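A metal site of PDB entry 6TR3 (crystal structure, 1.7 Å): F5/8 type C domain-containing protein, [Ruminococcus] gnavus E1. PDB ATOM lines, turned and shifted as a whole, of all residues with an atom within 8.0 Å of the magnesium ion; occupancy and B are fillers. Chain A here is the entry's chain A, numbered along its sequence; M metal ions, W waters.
OG of Ser 107 sits close to N of His 109 (3.2 Å).
The side-chain hydroxyl (OG) of Ser 107 sits at hydrogen-bond distance from the side-chain carboxylate (OE1) of Glu 186 (2.6 Å).
The side-chain amide nitrogen of Gln 183 lies within hydrogen-bond range of the side-chain hydroxyl of Ser 107, 3.3 Å away.
OG1 of Thr 110 is in hydrogen-bond range of N of Tyr 112, 2.9 Å away.
The backbone NH (N) of Lys 115 lies close to the side-chain carboxylate (OD1) of Asp 113 (3.2 Å).
The side-chain carboxylate (OD1) of Asp 113 lies within hydrogen-bond range of the backbone NH (N) of Ala 116.
The magnesium ion is bound by O of Ser 107 (2.1 Å), O of Thr 110 (2.1 Å), water W1 (2.1 Å), water W2 (2.1 Å), water W3 (2.1 Å) and OD2 of Asp 113 (2.2 Å).
The magnesium ion has six donor atoms within binding distance.
Merely in contact with the magnesium ion: Glu 111 (3.97 Å).
Of the 15 residues printed, 4 come within 4 Å of the magnesium ion.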
ATOM      1  N   CYS A 103      16.795 -14.742 -20.750  1.00  0.00           N
ATOM      2  CA  CYS A 103      17.636 -14.931 -21.926  1.00  0.00           C
ATOM      3  C   CYS A 103      17.309 -16.262 -22.604  1.00  0.00           C
ATOM      4  O   CYS A 103      17.297 -17.306 -21.950  1.00  0.00           O
ATOM      5  CB  CYS A 103      19.101 -14.870 -21.510  1.00  0.00           C
ATOM      6  SG  CYS A 103      19.488 -13.211 -20.903  1.00  0.00           S
ATOM      7  N   TRP A 105      19.139 -17.812 -24.798  1.00  0.00           N
ATOM      8  CA  TRP A 105      20.359 -18.529 -25.146  1.00  0.00           C
ATOM      9  C   TRP A 105      21.002 -19.005 -23.857  1.00  0.00           C
ATOM     10  O   TRP A 105      20.632 -18.547 -22.766  1.00  0.00           O
ATOM     11  CB  TRP A 105      21.314 -17.676 -26.011  1.00  0.00           C
ATOM     12  CG  TRP A 105      22.140 -16.666 -25.264  1.00  0.00           C
ATOM     13  CD1 TRP A 105      23.445 -16.808 -24.869  1.00  0.00           C
ATOM     14  CD2 TRP A 105      21.722 -15.382 -24.800  1.00  0.00           C
ATOM     15  NE1 TRP A 105      23.851 -15.700 -24.192  1.00  0.00           N
ATOM     16  CE2 TRP A 105      22.816 -14.802 -24.123  1.00  0.00           C
ATOM     17  CE3 TRP A 105      20.527 -14.638 -24.899  1.00  0.00           C
ATOM     18  CZ2 TRP A 105      22.749 -13.541 -23.541  1.00  0.00           C
ATOM     19  CZ3 TRP A 105      20.463 -13.383 -24.287  1.00  0.00           C
ATOM     20  CH2 TRP A 105      21.587 -12.856 -23.623  1.00  0.00           C
ATOM     21  N   ASP A 106      21.945 -19.941 -23.970  1.00  0.00           N
ATOM     22  CA  ASP A 106      22.641 -20.485 -22.791  1.00  0.00           C
ATOM     23  C   ASP A 106      23.734 -19.497 -22.371  1.00  0.00           C
ATOM     24  O   ASP A 106      24.843 -19.511 -22.929  1.00  0.00           O
ATOM     25  CB  ASP A 106      23.186 -21.881 -23.104  1.00  0.00           C
ATOM     26  CG  ASP A 106      23.956 -22.494 -21.959  1.00  0.00           C
ATOM     27  OD1 ASP A 106      24.166 -21.815 -20.948  1.00  0.00           O
ATOM     28  OD2 ASP A 106      24.348 -23.672 -22.091  1.00  0.00           O
ATOM     29  N   SER A 107      23.410 -18.598 -21.428  1.00  0.00           N
ATOM     30  CA  SER A 107      24.323 -17.561 -20.958  1.00  0.00           C
ATOM     31  C   SER A 107      25.022 -17.894 -19.654  1.00  0.00           C
ATOM     32  O   SER A 107      24.384 -18.157 -18.647  1.00  0.00           O
ATOM     33  CB  SER A 107      23.593 -16.256 -20.749  1.00  0.00           C
ATOM     34  OG  SER A 107      24.514 -15.220 -20.446  1.00  0.00           O
ATOM     35  N   GLU A 108      26.355 -17.774 -19.649  1.00  0.00           N
ATOM     36  CA  GLU A 108      27.141 -17.931 -18.426  1.00  0.00           C
ATOM     37  C   GLU A 108      27.056 -16.721 -17.494  1.00  0.00           C
ATOM     38  O   GLU A 108      27.544 -16.790 -16.377  1.00  0.00           O
ATOM     39  CB  GLU A 108      28.615 -18.200 -18.774  1.00  0.00           C
ATOM     40  CG  GLU A 108      29.416 -16.963 -19.193  1.00  0.00           C
ATOM     41  CD  GLU A 108      30.882 -17.263 -19.485  1.00  0.00           C
ATOM     42  OE1 GLU A 108      31.177 -18.073 -20.385  1.00  0.00           O
ATOM     43  OE2 GLU A 108      31.758 -16.683 -18.797  1.00  0.00           O
ATOM     44  N   HIS A 109      26.435 -15.626 -17.941  1.00  0.00           N
ATOM     45  CA  HIS A 109      26.381 -14.379 -17.172  1.00  0.00           C
ATOM     46  C   HIS A 109      25.099 -14.216 -16.372  1.00  0.00           C
ATOM     47  O   HIS A 109      24.970 -13.285 -15.603  1.00  0.00           O
ATOM     48  CB  HIS A 109      26.603 -13.179 -18.088  1.00  0.00           C
ATOM     49  CG  HIS A 109      27.900 -13.231 -18.821  1.00  0.00           C
ATOM     50  ND1 HIS A 109      29.118 -13.115 -18.170  1.00  0.00           N
ATOM     51  CD2 HIS A 109      28.182 -13.416 -20.126  1.00  0.00           C
ATOM     52  CE1 HIS A 109      30.094 -13.216 -19.065  1.00  0.00           C
ATOM     53  NE2 HIS A 109      29.553 -13.396 -20.256  1.00  0.00           N
ATOM     54  N   THR A 110      24.147 -15.145 -16.564  1.00  0.00           N
ATOM     55  CA  THR A 110      22.947 -15.190 -15.746  1.00  0.00           C
ATOM     56  C   THR A 110      22.417 -16.603 -15.622  1.00  0.00           C
ATOM     57  O   THR A 110      22.599 -17.436 -16.527  1.00  0.00           O
ATOM     58  CB  THR A 110      21.839 -14.280 -16.339  1.00  0.00           C
ATOM     59  OG1 THR A 110      20.699 -14.234 -15.465  1.00  0.00           O
ATOM     60  CG2 THR A 110      21.384 -14.785 -17.692  1.00  0.00           C
ATOM     61  N   GLU A 111      21.710 -16.852 -14.519  1.00  0.00           N
ATOM     62  CA  GLU A 111      20.928 -18.067 -14.350  1.00  0.00           C
ATOM     63  C   GLU A 111      19.473 -17.915 -14.829  1.00  0.00           C
ATOM     64  O   GLU A 111      18.724 -18.891 -14.819  1.00  0.00           O
ATOM     65  CB  GLU A 111      20.985 -18.534 -12.890  1.00  0.00           C
ATOM     66  CG  GLU A 111      22.375 -19.011 -12.523  1.00  0.00           C
ATOM     67  CD  GLU A 111      22.436 -19.604 -11.133  1.00  0.00           C
ATOM     68  OE1 GLU A 111      22.329 -18.828 -10.161  1.00  0.00           O
ATOM     69  OE2 GLU A 111      22.586 -20.838 -11.021  1.00  0.00           O
ATOM     70  N   TYR A 112      19.111 -16.709 -15.295  1.00  0.00           N
ATOM     71  CA  TYR A 112      17.739 -16.422 -15.723  1.00  0.00           C
ATOM     72  C   TYR A 112      17.639 -16.652 -17.209  1.00  0.00           C
ATOM     73  O   TYR A 112      17.440 -15.712 -17.991  1.00  0.00           O
ATOM     74  CB  TYR A 112      17.347 -14.976 -15.352  1.00  0.00           C
ATOM     75  CG  TYR A 112      15.854 -14.678 -15.217  1.00  0.00           C
ATOM     76  CD1 TYR A 112      15.058 -15.347 -14.307  1.00  0.00           C
ATOM     77  CD2 TYR A 112      15.284 -13.633 -15.938  1.00  0.00           C
ATOM     78  CE1 TYR A 112      13.720 -15.040 -14.150  1.00  0.00           C
ATOM     79  CE2 TYR A 112      13.952 -13.298 -15.779  1.00  0.00           C
ATOM     80  CZ  TYR A 112      13.174 -13.996 -14.889  1.00  0.00           C
ATOM     81  OH  TYR A 112      11.840 -13.635 -14.749  1.00  0.00           O
ATOM     82  N   ASP A 113      17.781 -17.918 -17.603  1.00  0.00           N
ATOM     83  CA  ASP A 113      17.816 -18.271 -18.992  1.00  0.00           C
ATOM     84  C   ASP A 113      17.219 -19.638 -19.303  1.00  0.00           C
ATOM     85  O   ASP A 113      16.827 -20.391 -18.416  1.00  0.00           O
ATOM     86  CB  ASP A 113      19.258 -18.145 -19.527  1.00  0.00           C
ATOM     87  CG  ASP A 113      20.236 -19.114 -18.861  1.00  0.00           C
ATOM     88  OD1 ASP A 113      19.766 -20.133 -18.319  1.00  0.00           O
ATOM     89  OD2 ASP A 113      21.467 -18.851 -18.916  1.00  0.00           O
ATOM     90  N   VAL A 114      17.169 -19.928 -20.602  1.00  0.00           N
ATOM     91  CA  VAL A 114      16.568 -21.152 -21.103  1.00  0.00           C
ATOM     92  C   VAL A 114      17.275 -22.407 -20.567  1.00  0.00           C
ATOM     93  O   VAL A 114      16.641 -23.416 -20.372  1.00  0.00           O
ATOM     94  CB  VAL A 114      16.476 -21.146 -22.650  1.00  0.00           C
ATOM     95  CG1 VAL A 114      17.843 -20.940 -23.285  1.00  0.00           C
ATOM     96  CG2 VAL A 114      15.809 -22.414 -23.181  1.00  0.00           C
ATOM     97  N   LYS A 115      18.586 -22.305 -20.322  1.00  0.00           N
ATOM     98  CA  LYS A 115      19.393 -23.427 -19.833  1.00  0.00           C
ATOM     99  C   LYS A 115      18.894 -23.880 -18.476  1.00  0.00           C
ATOM    100  O   LYS A 115      18.825 -25.060 -18.219  1.00  0.00           O
ATOM    101  CB  LYS A 115      20.880 -23.073 -19.802  1.00  0.00           C
ATOM    102  CG  LYS A 115      21.816 -24.180 -19.305  1.00  0.00           C
ATOM    103  CD  LYS A 115      21.887 -25.319 -20.311  1.00  0.00           C
ATOM    104  CE  LYS A 115      23.013 -26.283 -19.974  1.00  0.00           C
ATOM    105  NZ  LYS A 115      22.722 -27.056 -18.739  1.00  0.00           N
ATOM    106  N   ALA A 116      18.534 -22.911 -17.625  1.00  0.00           N
ATOM    107  CA  ALA A 116      17.980 -23.161 -16.295  1.00  0.00           C
ATOM    108  C   ALA A 116      16.524 -23.594 -16.284  1.00  0.00           C
ATOM    109  O   ALA A 116      16.040 -24.072 -15.248  1.00  0.00           O
ATOM    110  CB  ALA A 116      18.145 -21.923 -15.426  1.00  0.00           C
ATOM    111  N   GLN A 183      27.184  -9.876 -22.328  1.00  0.00           N
ATOM    112  CA  GLN A 183      26.204 -10.632 -23.083  1.00  0.00           C
ATOM    113  C   GLN A 183      26.345 -10.369 -24.588  1.00  0.00           C
ATOM    114  O   GLN A 183      26.196 -11.295 -25.387  1.00  0.00           O
ATOM    115  CB  GLN A 183      24.784 -10.407 -22.587  1.00  0.00           C
ATOM    116  CG  GLN A 183      24.537 -11.141 -21.273  1.00  0.00           C
ATOM    117  CD  GLN A 183      23.074 -11.320 -20.913  1.00  0.00           C
ATOM    118  OE1 GLN A 183      22.217 -10.470 -21.208  1.00  0.00           O
ATOM    119  NE2 GLN A 183      22.763 -12.445 -20.259  1.00  0.00           N
ATOM    120  N   GLU A 186      29.322 -12.389 -25.601  1.00  0.00           N
ATOM    121  CA  GLU A 186      28.999 -13.821 -25.507  1.00  0.00           C
ATOM    122  C   GLU A 186      28.258 -14.296 -26.757  1.00  0.00           C
ATOM    123  O   GLU A 186      28.553 -15.354 -27.300  1.00  0.00           O
ATOM    124  CB  GLU A 186      28.176 -14.100 -24.227  1.00  0.00           C
ATOM    125  CG  GLU A 186      27.911 -15.564 -24.001  1.00  0.00           C
ATOM    126  CD  GLU A 186      27.114 -15.844 -22.775  1.00  0.00           C
ATOM    127  OE1 GLU A 186      26.120 -15.114 -22.527  1.00  0.00           O
ATOM    128  OE2 GLU A 186      27.487 -16.804 -22.050  1.00  0.00           O
HETATM  129 MG    MG M   1      23.046 -19.225 -17.505  1.00  0.00          MG
HETATM  130  O   HOH W   1      23.605 -21.011 -18.453  1.00  0.00           O
HETATM  131  O   HOH W   2      24.518 -19.536 -16.044  1.00  0.00           O
HETATM  132  O   HOH W   3      21.651 -20.412 -16.436  1.00  0.00           O
